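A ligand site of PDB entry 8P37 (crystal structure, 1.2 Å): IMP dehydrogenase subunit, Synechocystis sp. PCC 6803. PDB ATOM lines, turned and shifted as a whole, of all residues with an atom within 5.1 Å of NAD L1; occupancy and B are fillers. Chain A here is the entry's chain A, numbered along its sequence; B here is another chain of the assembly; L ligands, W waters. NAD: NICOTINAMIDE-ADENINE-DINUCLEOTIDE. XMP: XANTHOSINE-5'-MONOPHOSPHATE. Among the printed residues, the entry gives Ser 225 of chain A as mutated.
N7N of NAD L1 sits at hydrogen-bond distance from O2' of XMP L2 (3.3 Å).
Water W15 lies within hydrogen-bond range of O2B of NAD L1 (2.5 Å) and O of Leu 32 of chain B (2.7 Å). Water W5 lies within hydrogen-bond range of an oxygen (O3D) of NAD L1 (2.6 Å), the side-chain amide oxygen (OE1) of Gln 163 (2.8 Å), the side-chain hydroxyl (OG) of Ser 139 (3.0 Å) and the side-chain amide nitrogen (ND2) of Asn 79 (3.5 Å). Water W8 bridges an oxygen (O2A) of NAD L1 (2.7 Å) and the side-chain hydroxyl of Thr 141 (3.0 Å). Water W9 lies within hydrogen-bond range of an oxygen (O1A) of NAD L1 (2.9 Å) and the guanidinium group (NH1) of Arg 314 (3.4 Å). Water W3 lies within hydrogen-bond range of an oxygen (O4B) of NAD L1 (2.9 Å) and the backbone NH (N) of Val 143 (3.0 Å). Water W16 lies within hydrogen-bond range of O of Ser 168 (3.0 Å), N of His 171 (3.3 Å), O of Leu 180 (3.3 Å) and N6A of NAD L1 (3.3 Å).
The backbone NH of Ser 168 is in hydrogen-bond range of a nitrogen (N7A) of NAD L1 (3.1 Å). The backbone NH (N) of Ala 306 sits at hydrogen-bond distance from an oxygen (O6) of XMP L2. OD1 of Asp 264 sits at hydrogen-bond distance from O3' of XMP L2. N of Gly 220 sits at hydrogen-bond distance from O7N of NAD L1 (2.8 Å). An oxygen (O2) of XMP L2 sits at hydrogen-bond distance from the side-chain hydroxyl (OG) of Ser 227, 2.7 Å away. A nitrogen (N1) of XMP L2 sits at hydrogen-bond distance from the backbone carbonyl oxygen (O) of Arg 314. The backbone carbonyl oxygen (O) of Ser 168 is in hydrogen-bond range of a nitrogen (N6A) of NAD L1, at 3.1 Å. O2 of XMP L2 sits at hydrogen-bond distance from OG of Ser 225, 2.5 Å away. N6A of NAD L1 lies within hydrogen-bond range of O of Leu 180 (3.0 Å). The side-chain amide nitrogen (ND2) of Asn 79 lies within hydrogen-bond range of an oxygen (O3D) of NAD L1. The backbone NH (N) of Thr 165 is in hydrogen-bond range of an oxygen (O1N) of NAD L1, 2.8 Å away. The guanidinium group (NH1) of Arg 314 lies within salt-bridge range of an oxygen (O2N) of NAD L1, at 2.8 Å. The backbone NH of Leu 180 sits at hydrogen-bond distance from a nitrogen (N1A) of NAD L1 (3.0 Å). The side-chain hydroxyl (OG1) of Thr 165 is in hydrogen-bond range of an oxygen (O1N) of NAD L1, 2.6 Å away. O of Gly 218 lies within hydrogen-bond range of N7N of NAD L1 (3.2 Å). The backbone NH (N) of Met 305 sits at hydrogen-bond distance from a nitrogen (N7) of XMP L2.
Merely in contact with NAD L1: Ala 56, Thr 141, Pro 142, Gln 163, Ala 164, Val 166, Val 167, His 171, Ser 179, Asn 197, Ile 219, Ser 227, Met 305 and Ala 306.
The backbone carbonyl oxygen (O) of His 171 sits close to the side-chain hydroxyl (OG) of Ser 179, 3.4 Å away. O of Ala 164 sits at hydrogen-bond distance from N of Asn 197 (2.9 Å). N of Ser 227 is in hydrogen-bond range of OG of Ser 225. The backbone NH of Ser 227 is in hydrogen-bond range of the backbone carbonyl oxygen of Arg 314 (3.4 Å). The side-chain carboxylate (OD2) of Asp 264 is in hydrogen-bond range of the side-chain amide nitrogen (NE2) of Gln 163. The side-chain hydroxyl of Ser 225 sits at hydrogen-bond distance from the backbone carbonyl oxygen of Gly 220 (3.3 Å). The backbone carbonyl oxygen (O) of Ala 306 sits at hydrogen-bond distance from the backbone NH (N) of Arg 314. The side-chain amide oxygen (OD1) of Asn 197 is in hydrogen-bond range of the side-chain amide nitrogen (NE2) of Gln 163 (3.0 Å).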
ATOM      1  N   ALA A  56     -30.900   1.713 -31.602  1.00  0.00           N
ATOM      2  CA  ALA A  56     -32.193   1.737 -30.899  1.00  0.00           C
ATOM      3  C   ALA A  56     -32.233   2.960 -29.960  1.00  0.00           C
ATOM      4  O   ALA A  56     -32.087   2.826 -28.728  1.00  0.00           O
ATOM      5  CB  ALA A  56     -32.441   0.447 -30.147  1.00  0.00           C
ATOM      6  N   ASN A  79     -36.361   1.009 -30.020  1.00  0.00           N
ATOM      7  CA  ASN A  79     -36.207   0.753 -28.579  1.00  0.00           C
ATOM      8  C   ASN A  79     -37.548   0.579 -27.905  1.00  0.00           C
ATOM      9  O   ASN A  79     -38.321   1.554 -27.822  1.00  0.00           O
ATOM     10  CB  ASN A  79     -35.412   1.869 -27.941  1.00  0.00           C
ATOM     11  CG  ASN A  79     -34.803   1.454 -26.635  1.00  0.00           C
ATOM     12  OD1 ASN A  79     -35.475   0.937 -25.756  1.00  0.00           O
ATOM     13  ND2 ASN A  79     -33.530   1.661 -26.475  1.00  0.00           N
ATOM     14  N   SER A 139     -35.557  -3.629 -29.595  1.00  0.00           N
ATOM     15  CA  SER A 139     -34.655  -3.858 -28.465  1.00  0.00           C
ATOM     16  C   SER A 139     -35.328  -3.792 -27.109  1.00  0.00           C
ATOM     17  O   SER A 139     -36.293  -3.026 -26.907  1.00  0.00           O
ATOM     18  CB  SER A 139     -33.451  -2.924 -28.481  1.00  0.00           C
ATOM     19  OG  SER A 139     -33.850  -1.588 -28.192  1.00  0.00           O
ATOM     20  N   THR A 141     -33.777  -4.124 -22.773  1.00  0.00           N
ATOM     21  CA  THR A 141     -32.740  -4.446 -21.806  1.00  0.00           C
ATOM     22  C   THR A 141     -33.056  -5.852 -21.233  1.00  0.00           C
ATOM     23  O   THR A 141     -34.172  -6.353 -21.408  1.00  0.00           O
ATOM     24  CB  THR A 141     -32.728  -3.445 -20.628  1.00  0.00           C
ATOM     25  OG1 THR A 141     -33.991  -3.509 -19.936  1.00  0.00           O
ATOM     26  CG2 THR A 141     -32.392  -2.026 -21.052  1.00  0.00           C
ATOM     27  N   PRO A 142     -32.100  -6.534 -20.563  1.00  0.00           N
ATOM     28  CA  PRO A 142     -32.401  -7.848 -19.985  1.00  0.00           C
ATOM     29  C   PRO A 142     -33.646  -7.871 -19.057  1.00  0.00           C
ATOM     30  O   PRO A 142     -34.515  -8.713 -19.239  1.00  0.00           O
ATOM     31  CB  PRO A 142     -31.115  -8.159 -19.247  1.00  0.00           C
ATOM     32  CG  PRO A 142     -30.066  -7.489 -20.023  1.00  0.00           C
ATOM     33  CD  PRO A 142     -30.664  -6.188 -20.409  1.00  0.00           C
ATOM     34  N   VAL A 143     -33.819  -6.857 -18.187  1.00  0.00           N
ATOM     35  CA  VAL A 143     -35.011  -6.755 -17.323  1.00  0.00           C
ATOM     36  C   VAL A 143     -36.263  -6.514 -18.176  1.00  0.00           C
ATOM     37  O   VAL A 143     -37.305  -7.125 -17.937  1.00  0.00           O
ATOM     38  CB  VAL A 143     -34.839  -5.670 -16.223  1.00  0.00           C
ATOM     39  CG1 VAL A 143     -36.148  -5.368 -15.507  1.00  0.00           C
ATOM     40  CG2 VAL A 143     -33.747  -6.075 -15.240  1.00  0.00           C
ATOM     41  N   GLN A 163     -30.182  -5.585 -25.420  1.00  0.00           N
ATOM     42  CA  GLN A 163     -29.059  -4.665 -25.406  1.00  0.00           C
ATOM     43  C   GLN A 163     -29.058  -3.821 -24.174  1.00  0.00           C
ATOM     44  O   GLN A 163     -30.036  -3.192 -23.790  1.00  0.00           O
ATOM     45  CB  GLN A 163     -29.161  -3.767 -26.658  1.00  0.00           C
ATOM     46  CG  GLN A 163     -28.020  -2.797 -26.764  1.00  0.00           C
ATOM     47  CD  GLN A 163     -27.958  -2.061 -28.070  1.00  0.00           C
ATOM     48  OE1 GLN A 163     -28.943  -1.592 -28.646  1.00  0.00           O
ATOM     49  NE2 GLN A 163     -26.734  -1.884 -28.530  1.00  0.00           N
ATOM     50  N   ALA A 164     -27.894  -3.744 -23.560  1.00  0.00           N
ATOM     51  CA  ALA A 164     -27.648  -2.828 -22.495  1.00  0.00           C
ATOM     52  C   ALA A 164     -26.145  -2.542 -22.440  1.00  0.00           C
ATOM     53  O   ALA A 164     -25.376  -3.110 -23.228  1.00  0.00           O
ATOM     54  CB  ALA A 164     -28.204  -3.370 -21.207  1.00  0.00           C
ATOM     55  N   THR A 165     -25.674  -1.718 -21.505  1.00  0.00           N
ATOM     56  CA  THR A 165     -24.248  -1.405 -21.386  1.00  0.00           C
ATOM     57  C   THR A 165     -23.425  -2.696 -21.358  1.00  0.00           C
ATOM     58  O   THR A 165     -22.461  -2.830 -22.145  1.00  0.00           O
ATOM     59  CB  THR A 165     -23.967  -0.582 -20.128  1.00  0.00           C
ATOM     60  OG1 THR A 165     -24.776   0.567 -20.107  1.00  0.00           O
ATOM     61  CG2 THR A 165     -22.512  -0.229 -20.038  1.00  0.00           C
ATOM     62  N   VAL A 166     -23.865  -3.650 -20.512  1.00  0.00           N
ATOM     63  CA  VAL A 166     -23.405  -5.040 -20.455  1.00  0.00           C
ATOM     64  C   VAL A 166     -24.644  -5.956 -20.377  1.00  0.00           C
ATOM     65  O   VAL A 166     -25.644  -5.610 -19.779  1.00  0.00           O
ATOM     66  CB  VAL A 166     -22.427  -5.302 -19.288  1.00  0.00           C
ATOM     67  CG1 VAL A 166     -21.078  -4.623 -19.506  1.00  0.00           C
ATOM     68  CG2 VAL A 166     -23.034  -4.850 -17.952  1.00  0.00           C
ATOM     69  N   VAL A 167     -24.516  -7.145 -20.985  1.00  0.00           N
ATOM     70  CA  VAL A 167     -25.545  -8.180 -20.942  1.00  0.00           C
ATOM     71  C   VAL A 167     -24.757  -9.423 -20.623  1.00  0.00           C
ATOM     72  O   VAL A 167     -23.724  -9.705 -21.274  1.00  0.00           O
ATOM     73  CB  VAL A 167     -26.431  -8.248 -22.214  1.00  0.00           C
ATOM     74  CG1 VAL A 167     -27.219  -9.545 -22.331  1.00  0.00           C
ATOM     75  CG2 VAL A 167     -27.385  -7.042 -22.268  1.00  0.00           C
ATOM     76  N   SER A 168     -25.179 -10.162 -19.596  1.00  0.00           N
ATOM     77  CA  SER A 168     -24.383 -11.242 -19.067  1.00  0.00           C
ATOM     78  C   SER A 168     -25.134 -12.519 -18.926  1.00  0.00           C
ATOM     79  O   SER A 168     -26.284 -12.519 -18.498  1.00  0.00           O
ATOM     80  CB  SER A 168     -23.857 -10.812 -17.688  1.00  0.00           C
ATOM     81  OG  SER A 168     -22.926 -11.748 -17.173  1.00  0.00           O
ATOM     82  N   HIS A 171     -25.254 -12.859 -14.424  1.00  0.00           N
ATOM     83  CA  HIS A 171     -25.689 -11.668 -13.725  1.00  0.00           C
ATOM     84  C   HIS A 171     -26.236 -11.983 -12.338  1.00  0.00           C
ATOM     85  O   HIS A 171     -27.172 -12.796 -12.203  1.00  0.00           O
ATOM     86  CB  HIS A 171     -26.739 -10.914 -14.528  1.00  0.00           C
ATOM     87  CG  HIS A 171     -27.167  -9.652 -13.880  1.00  0.00           C
ATOM     88  ND1 HIS A 171     -26.315  -8.576 -13.770  1.00  0.00           N
ATOM     89  CD2 HIS A 171     -28.314  -9.358 -13.219  1.00  0.00           C
ATOM     90  CE1 HIS A 171     -26.980  -7.653 -13.092  1.00  0.00           C
ATOM     91  NE2 HIS A 171     -28.189  -8.077 -12.741  1.00  0.00           N
ATOM     92  N   GLU A 178     -35.975 -10.121 -11.604  1.00  0.00           N
ATOM     93  CA  GLU A 178     -35.855 -11.328 -12.381  1.00  0.00           C
ATOM     94  C   GLU A 178     -34.658 -11.229 -13.315  1.00  0.00           C
ATOM     95  O   GLU A 178     -34.733 -10.484 -14.294  1.00  0.00           O
ATOM     96  CB  GLU A 178     -37.144 -11.571 -13.194  1.00  0.00           C
ATOM     97  N   SER A 179     -33.568 -11.974 -13.035  1.00  0.00           N
ATOM     98  CA  SER A 179     -32.423 -11.979 -13.949  1.00  0.00           C
ATOM     99  C   SER A 179     -32.846 -12.769 -15.156  1.00  0.00           C
ATOM    100  O   SER A 179     -33.569 -13.758 -15.048  1.00  0.00           O
ATOM    101  CB  SER A 179     -31.184 -12.665 -13.377  1.00  0.00           C
ATOM    102  OG  SER A 179     -30.371 -11.836 -12.579  1.00  0.00           O
ATOM    103  N   LEU A 180     -32.343 -12.369 -16.307  1.00  0.00           N
ATOM    104  CA  LEU A 180     -32.730 -13.021 -17.557  1.00  0.00           C
ATOM    105  C   LEU A 180     -31.782 -14.175 -17.875  1.00  0.00           C
ATOM    106  O   LEU A 180     -30.569 -13.986 -17.910  1.00  0.00           O
ATOM    107  CB  LEU A 180     -32.706 -11.982 -18.628  1.00  0.00           C
ATOM    108  CG  LEU A 180     -33.081 -12.436 -20.049  1.00  0.00           C
ATOM    109  CD1 LEU A 180     -34.567 -12.797 -20.136  1.00  0.00           C
ATOM    110  CD2 LEU A 180     -32.766 -11.358 -21.022  1.00  0.00           C
ATOM    111  N   LEU A 182     -30.329 -16.011 -20.594  1.00  0.00           N
ATOM    112  CA  LEU A 182     -30.125 -15.787 -22.015  1.00  0.00           C
ATOM    113  C   LEU A 182     -30.198 -17.071 -22.802  1.00  0.00           C
ATOM    114  O   LEU A 182     -30.598 -17.047 -23.973  1.00  0.00           O
ATOM    115  CB  LEU A 182     -28.800 -15.079 -22.265  1.00  0.00           C
ATOM    116  CG  LEU A 182     -28.656 -13.702 -21.619  1.00  0.00           C
ATOM    117  CD1 LEU A 182     -27.260 -13.234 -21.721  1.00  0.00           C
ATOM    118  CD2 LEU A 182     -29.617 -12.684 -22.214  1.00  0.00           C
ATOM    119  N   ASN A 197     -24.249  -5.294 -24.820  1.00  0.00           N
ATOM    120  CA  ASN A 197     -22.981  -5.067 -25.454  1.00  0.00           C
ATOM    121  C   ASN A 197     -21.862  -5.743 -24.659  1.00  0.00           C
ATOM    122  O   ASN A 197     -22.011  -6.068 -23.473  1.00  0.00           O
ATOM    123  CB  ASN A 197     -22.752  -3.555 -25.627  1.00  0.00           C
ATOM    124  CG  ASN A 197     -23.507  -2.970 -26.760  1.00  0.00           C
ATOM    125  OD1 ASN A 197     -24.653  -3.389 -27.014  1.00  0.00           O
ATOM    126  ND2 ASN A 197     -22.928  -2.101 -27.537  1.00  0.00           N
ATOM    127  N   GLY A 218     -19.198  -2.771 -27.954  1.00  0.00           N
ATOM    128  CA  GLY A 218     -18.920  -1.370 -27.660  1.00  0.00           C
ATOM    129  C   GLY A 218     -19.478  -0.924 -26.338  1.00  0.00           C
ATOM    130  O   GLY A 218     -20.672  -1.106 -26.052  1.00  0.00           O
ATOM    131  N   ILE A 219     -18.630  -0.331 -25.500  1.00  0.00           N
ATOM    132  CA  ILE A 219     -19.042   0.263 -24.244  1.00  0.00           C
ATOM    133  C   ILE A 219     -18.545   1.686 -24.238  1.00  0.00           C
ATOM    134  O   ILE A 219     -17.339   1.905 -24.144  1.00  0.00           O
ATOM    135  CB  ILE A 219     -18.580  -0.523 -22.983  1.00  0.00           C
ATOM    136  CG1 ILE A 219     -19.281  -1.905 -22.923  1.00  0.00           C
ATOM    137  CG2 ILE A 219     -18.924   0.293 -21.713  1.00  0.00           C
ATOM    138  CD1 ILE A 219     -18.646  -2.865 -21.960  1.00  0.00           C
ATOM    139  N   GLY A 220     -19.451   2.645 -24.353  1.00  0.00           N
ATOM    140  CA  GLY A 220     -19.097   4.040 -24.308  1.00  0.00           C
ATOM    141  C   GLY A 220     -18.510   4.776 -25.484  1.00  0.00           C
ATOM    142  O   GLY A 220     -18.200   5.930 -25.269  1.00  0.00           O
ATOM    143  N   PRO A 221     -18.307   4.218 -26.714  1.00  0.00           N
ATOM    144  CA  PRO A 221     -17.783   5.064 -27.797  1.00  0.00           C
ATOM    145  C   PRO A 221     -18.783   6.084 -28.338  1.00  0.00           C
ATOM    146  O   PRO A 221     -18.389   6.917 -29.132  1.00  0.00           O
ATOM    147  CB  PRO A 221     -17.399   4.040 -28.849  1.00  0.00           C
ATOM    148  CG  PRO A 221     -18.451   2.939 -28.703  1.00  0.00           C
ATOM    149  CD  PRO A 221     -18.617   2.854 -27.183  1.00  0.00           C
ATOM    150  N   SER A 225     -22.846   9.335 -25.599  1.00  0.00           N
ATOM    151  CA  SER A 225     -22.539   8.511 -24.470  1.00  0.00           C
ATOM    152  C   SER A 225     -21.725   9.251 -23.446  1.00  0.00           C
ATOM    153  O   SER A 225     -20.763   9.923 -23.787  1.00  0.00           O
ATOM    154  CB  SER A 225     -21.698   7.347 -24.948  1.00  0.00           C
ATOM    155  OG  SER A 225     -21.113   6.638 -23.863  1.00  0.00           O
ATOM    156  N   SER A 227     -21.046   7.178 -20.465  1.00  0.00           N
ATOM    157  CA  SER A 227     -20.669   6.071 -19.587  1.00  0.00           C
ATOM    158  C   SER A 227     -19.211   5.983 -19.232  1.00  0.00           C
ATOM    159  O   SER A 227     -18.868   5.598 -18.106  1.00  0.00           O
ATOM    160  CB  SER A 227     -21.090   4.725 -20.149  1.00  0.00           C
ATOM    161  OG  SER A 227     -22.508   4.631 -20.259  1.00  0.00           O
ATOM    162  N   ASP A 264     -20.599  -1.281 -32.538  1.00  0.00           N
ATOM    163  CA  ASP A 264     -21.669  -0.380 -32.183  1.00  0.00           C
ATOM    164  C   ASP A 264     -21.229   0.946 -31.589  1.00  0.00           C
ATOM    165  O   ASP A 264     -20.732   1.004 -30.460  1.00  0.00           O
ATOM    166  CB  ASP A 264     -22.563  -1.110 -31.161  1.00  0.00           C
ATOM    167  CG  ASP A 264     -23.733  -0.309 -30.659  1.00  0.00           C
ATOM    168  OD1 ASP A 264     -24.030   0.717 -31.250  1.00  0.00           O
ATOM    169  OD2 ASP A 264     -24.376  -0.738 -29.653  1.00  0.00           O
ATOM    170  N   MET A 305     -29.840   6.884 -24.586  1.00  0.00           N
ATOM    171  CA  MET A 305     -31.011   6.256 -23.946  1.00  0.00           C
ATOM    172  C   MET A 305     -30.835   5.994 -22.466  1.00  0.00           C
ATOM    173  O   MET A 305     -31.812   5.619 -21.851  1.00  0.00           O
ATOM    174  CB  MET A 305     -31.402   4.974 -24.703  1.00  0.00           C
ATOM    175  CG  MET A 305     -31.905   5.256 -26.143  1.00  0.00           C
ATOM    176  SD  MET A 305     -33.354   6.311 -26.218  1.00  0.00           S
ATOM    177  CE  MET A 305     -34.555   5.129 -25.731  1.00  0.00           C
ATOM    178  N   ALA A 306     -29.674   6.317 -21.875  1.00  0.00           N
ATOM    179  CA  ALA A 306     -29.503   6.357 -20.437  1.00  0.00           C
ATOM    180  C   ALA A 306     -29.463   7.791 -19.900  1.00  0.00           C
ATOM    181  O   ALA A 306     -29.345   7.982 -18.691  1.00  0.00           O
ATOM    182  CB  ALA A 306     -28.291   5.594 -20.014  1.00  0.00           C
ATOM    183  N   ARG A 314     -26.342   8.474 -17.900  1.00  0.00           N
ATOM    184  CA  ARG A 314     -25.117   8.017 -18.556  1.00  0.00           C
ATOM    185  C   ARG A 314     -25.120   8.281 -20.063  1.00  0.00           C
ATOM    186  O   ARG A 314     -24.379   7.685 -20.835  1.00  0.00           O
ATOM    187  CB  ARG A 314     -24.915   6.540 -18.258  1.00  0.00           C
ATOM    188  CG  ARG A 314     -24.447   6.295 -16.820  1.00  0.00           C
ATOM    189  CD  ARG A 314     -24.710   4.892 -16.334  1.00  0.00           C
ATOM    190  NE  ARG A 314     -26.167   4.761 -16.141  1.00  0.00           N
ATOM    191  CZ  ARG A 314     -27.019   4.099 -16.908  1.00  0.00           C
ATOM    192  NH1 ARG A 314     -26.578   3.296 -17.875  1.00  0.00           N
ATOM    193  NH2 ARG A 314     -28.325   4.129 -16.641  1.00  0.00           N
ATOM    194  N   THR B  31     -21.569  -9.938 -13.998  1.00  0.00           N
ATOM    195  CA  THR B  31     -22.040  -8.610 -13.680  1.00  0.00           C
ATOM    196  C   THR B  31     -22.896  -8.704 -12.436  1.00  0.00           C
ATOM    197  O   THR B  31     -23.387  -9.790 -12.114  1.00  0.00           O
ATOM    198  CB  THR B  31     -22.853  -8.026 -14.808  1.00  0.00           C
ATOM    199  OG1 THR B  31     -23.910  -8.906 -15.169  1.00  0.00           O
ATOM    200  CG2 THR B  31     -22.037  -7.754 -16.052  1.00  0.00           C
ATOM    201  N   LEU B  32     -23.126  -7.573 -11.739  1.00  0.00           N
ATOM    202  CA  LEU B  32     -23.979  -7.612 -10.554  1.00  0.00           C
ATOM    203  C   LEU B  32     -24.749  -6.348 -10.451  1.00  0.00           C
ATOM    204  O   LEU B  32     -24.312  -5.270 -10.898  1.00  0.00           O
ATOM    205  CB  LEU B  32     -23.193  -7.976  -9.282  1.00  0.00           C
ATOM    206  CG  LEU B  32     -21.940  -7.195  -8.906  1.00  0.00           C
ATOM    207  CD1 LEU B  32     -22.226  -6.048  -8.003  1.00  0.00           C
ATOM    208  CD2 LEU B  32     -20.917  -8.078  -8.164  1.00  0.00           C
ATOM    209  N   ASP B  33     -25.897  -6.437  -9.798  1.00  0.00           N
ATOM    210  CA  ASP B  33     -26.734  -5.277  -9.572  1.00  0.00           C
ATOM    211  C   ASP B  33     -25.932  -4.294  -8.693  1.00  0.00           C
ATOM    212  O   ASP B  33     -25.343  -4.735  -7.716  1.00  0.00           O
ATOM    213  CB  ASP B  33     -27.995  -5.692  -8.821  1.00  0.00           C
ATOM    214  CG  ASP B  33     -29.071  -4.658  -8.697  1.00  0.00           C
ATOM    215  OD1 ASP B  33     -28.850  -3.689  -7.981  1.00  0.00           O
ATOM    216  OD2 ASP B  33     -30.178  -4.883  -9.246  1.00  0.00           O
ATOM    217  N   PRO B  34     -25.928  -2.995  -8.996  1.00  0.00           N
ATOM    218  CA  PRO B  34     -25.182  -2.051  -8.167  1.00  0.00           C
ATOM    219  C   PRO B  34     -25.536  -2.093  -6.685  1.00  0.00           C
ATOM    220  O   PRO B  34     -24.677  -1.825  -5.854  1.00  0.00           O
ATOM    221  CB  PRO B  34     -25.547  -0.689  -8.767  1.00  0.00           C
ATOM    222  CG  PRO B  34     -26.275  -0.938  -9.989  1.00  0.00           C
ATOM    223  CD  PRO B  34     -26.558  -2.333 -10.162  1.00  0.00           C
ATOM    224  N   THR B 353     -21.015  -3.297 -13.244  1.00  0.00           N
ATOM    225  CA  THR B 353     -20.679  -3.545 -14.643  1.00  0.00           C
ATOM    226  C   THR B 353     -19.482  -4.467 -14.765  1.00  0.00           C
ATOM    227  O   THR B 353     -19.398  -5.282 -15.705  1.00  0.00           O
ATOM    228  CB  THR B 353     -20.384  -2.222 -15.354  1.00  0.00           C
ATOM    229  OG1 THR B 353     -21.502  -1.343 -15.204  1.00  0.00           O
ATOM    230  CG2 THR B 353     -20.007  -2.351 -16.773  1.00  0.00           C
HETATM  231  PA  NAD L   1     -30.023  -0.560 -17.767  1.00  0.00           P
HETATM  232  O1A NAD L   1     -29.232   0.240 -16.861  1.00  0.00           O
HETATM  233  O2A NAD L   1     -31.493  -0.487 -17.601  1.00  0.00           O
HETATM  234  O5B NAD L   1     -29.696  -2.196 -17.784  1.00  0.00           O
HETATM  235  C5B NAD L   1     -28.402  -2.735 -17.766  1.00  0.00           C
HETATM  236  C4B NAD L   1     -28.160  -3.503 -16.608  1.00  0.00           C
HETATM  237  O4B NAD L   1     -28.770  -4.857 -16.795  1.00  0.00           O
HETATM  238  C3B NAD L   1     -26.647  -3.967 -16.510  1.00  0.00           C
HETATM  239  O3B NAD L   1     -25.862  -2.807 -15.968  1.00  0.00           O
HETATM  240  C2B NAD L   1     -26.670  -4.966 -15.689  1.00  0.00           C
HETATM  241  O2B NAD L   1     -26.738  -4.613 -14.230  1.00  0.00           O
HETATM  242  C1B NAD L   1     -28.091  -5.747 -16.068  1.00  0.00           C
HETATM  243  N9A NAD L   1     -27.887  -7.001 -16.745  1.00  0.00           N
HETATM  244  C8A NAD L   1     -26.935  -7.588 -17.447  1.00  0.00           C
HETATM  245  N7A NAD L   1     -27.306  -8.823 -17.746  1.00  0.00           N
HETATM  246  C5A NAD L   1     -28.475  -9.022 -17.126  1.00  0.00           C
HETATM  247  C6A NAD L   1     -29.203 -10.157 -17.027  1.00  0.00           C
HETATM  248  N6A NAD L   1     -29.026 -11.392 -17.714  1.00  0.00           N
HETATM  249  N1A NAD L   1     -30.342 -10.120 -16.351  1.00  0.00           N
HETATM  250  C2A NAD L   1     -30.735  -8.979 -15.721  1.00  0.00           C
HETATM  251  N3A NAD L   1     -29.966  -7.873 -15.769  1.00  0.00           N
HETATM  252  C4A NAD L   1     -28.837  -7.919 -16.462  1.00  0.00           C
HETATM  253  O3  NAD L   1     -29.700  -0.147 -19.267  1.00  0.00           O
HETATM  254  PN  NAD L   1     -28.483   0.651 -19.925  1.00  0.00           P
HETATM  255  O1N NAD L   1     -27.224  -0.156 -19.845  1.00  0.00           O
HETATM  256  O2N NAD L   1     -28.484   2.044 -19.429  1.00  0.00           O
HETATM  257  O5D NAD L   1     -28.966   0.650 -21.500  1.00  0.00           O
HETATM  258  C5D NAD L   1     -30.198   1.291 -21.802  1.00  0.00           C
HETATM  259  C4D NAD L   1     -30.186   1.791 -23.141  1.00  0.00           C
HETATM  260  O4D NAD L   1     -29.103   2.783 -23.417  1.00  0.00           O
HETATM  261  C3D NAD L   1     -29.924   0.706 -24.284  1.00  0.00           C
HETATM  262  O3D NAD L   1     -30.711   1.146 -25.495  1.00  0.00           O
HETATM  263  C2D NAD L   1     -28.594   0.731 -24.490  1.00  0.00           C
HETATM  264  O2D NAD L   1     -28.112   0.411 -25.863  1.00  0.00           O
HETATM  265  C1D NAD L   1     -28.109   2.256 -24.142  1.00  0.00           C
HETATM  266  N1N NAD L   1     -26.848   2.284 -23.429  1.00  0.00           N
HETATM  267  C2N NAD L   1     -25.740   1.839 -24.034  1.00  0.00           C
HETATM  268  C3N NAD L   1     -24.504   1.975 -23.415  1.00  0.00           C
HETATM  269  C7N NAD L   1     -23.230   1.478 -24.070  1.00  0.00           C
HETATM  270  O7N NAD L   1     -22.149   1.942 -23.765  1.00  0.00           O
HETATM  271  N7N NAD L   1     -23.296   0.522 -25.137  1.00  0.00           N
HETATM  272  C4N NAD L   1     -24.399   2.620 -22.226  1.00  0.00           C
HETATM  273  C5N NAD L   1     -25.519   3.114 -21.647  1.00  0.00           C
HETATM  274  C6N NAD L   1     -26.712   2.947 -22.266  1.00  0.00           C
HETATM  275  P   XMP L   2     -23.484   6.961 -31.738  1.00  0.00           P
HETATM  276  O1P XMP L   2     -24.000   6.669 -33.118  1.00  0.00           O
HETATM  277  O2P XMP L   2     -24.324   7.911 -30.946  1.00  0.00           O
HETATM  278  O5' XMP L   2     -23.506   5.524 -30.907  1.00  0.00           O
HETATM  279  O3P XMP L   2     -21.992   7.309 -31.722  1.00  0.00           O
HETATM  280  C5' XMP L   2     -24.721   4.905 -30.721  1.00  0.00           C
HETATM  281  C4' XMP L   2     -24.597   3.816 -29.668  1.00  0.00           C
HETATM  282  O4' XMP L   2     -24.444   4.452 -28.382  1.00  0.00           O
HETATM  283  C1' XMP L   2     -24.879   3.572 -27.384  1.00  0.00           C
HETATM  284  N9  XMP L   2     -25.758   4.319 -26.458  1.00  0.00           N
HETATM  285  C4  XMP L   2     -25.341   4.875 -25.299  1.00  0.00           C
HETATM  286  N3  XMP L   2     -24.130   4.770 -24.663  1.00  0.00           N
HETATM  287  N1  XMP L   2     -25.081   6.041 -22.940  1.00  0.00           N
HETATM  288  C2  XMP L   2     -24.016   5.317 -23.432  1.00  0.00           C
HETATM  289  O2  XMP L   2     -22.952   5.306 -22.815  1.00  0.00           O
HETATM  290  C6  XMP L   2     -26.296   6.208 -23.523  1.00  0.00           C
HETATM  291  O6  XMP L   2     -27.143   6.877 -22.944  1.00  0.00           O
HETATM  292  C5  XMP L   2     -26.423   5.500 -24.721  1.00  0.00           C
HETATM  293  N7  XMP L   2     -27.464   5.384 -25.636  1.00  0.00           N
HETATM  294  C8  XMP L   2     -27.029   4.693 -26.648  1.00  0.00           C
HETATM  295  C2' XMP L   2     -25.594   2.375 -28.060  1.00  0.00           C
HETATM  296  O2' XMP L   2     -24.628   1.293 -28.035  1.00  0.00           O
HETATM  297  C3' XMP L   2     -25.852   2.983 -29.458  1.00  0.00           C
HETATM  298  O3' XMP L   2     -26.041   2.013 -30.461  1.00  0.00           O
HETATM  299  O   HOH W   1     -21.585   4.141 -26.308  1.00  0.00           O
HETATM  300  O   HOH W   2     -23.884   2.844 -18.768  1.00  0.00           O
HETATM  301  O   HOH W   3     -31.612  -4.947 -17.556  1.00  0.00           O
HETATM  302  O   HOH W   4     -29.156   2.340 -27.692  1.00  0.00           O
HETATM  303  O   HOH W   5     -31.191  -0.788 -27.187  1.00  0.00           O
HETATM  304  O   HOH W   6     -23.751  -1.351 -16.735  1.00  0.00           O
HETATM  305  O   HOH W   7     -30.639  -5.735 -13.748  1.00  0.00           O
HETATM  306  O   HOH W   8     -33.159  -2.536 -17.263  1.00  0.00           O
HETATM  307  O   HOH W   9     -27.092   1.196 -15.238  1.00  0.00           O
HETATM  308  O   HOH W  10     -28.470  -4.261 -12.413  1.00  0.00           O
HETATM  309  O   HOH W  11     -30.738   3.269 -18.322  1.00  0.00           O
HETATM  310  O   HOH W  12     -26.548  -1.089 -13.888  1.00  0.00           O
HETATM  311  O   HOH W  13     -32.095   2.066 -16.183  1.00  0.00           O
HETATM  312  O   HOH W  14     -25.709  -1.002 -25.386  1.00  0.00           O
HETATM  313  O   HOH W  15     -24.386  -4.358 -13.433  1.00  0.00           O
HETATM  314  O   HOH W  16     -27.658 -14.087 -16.328  1.00  0.00           O
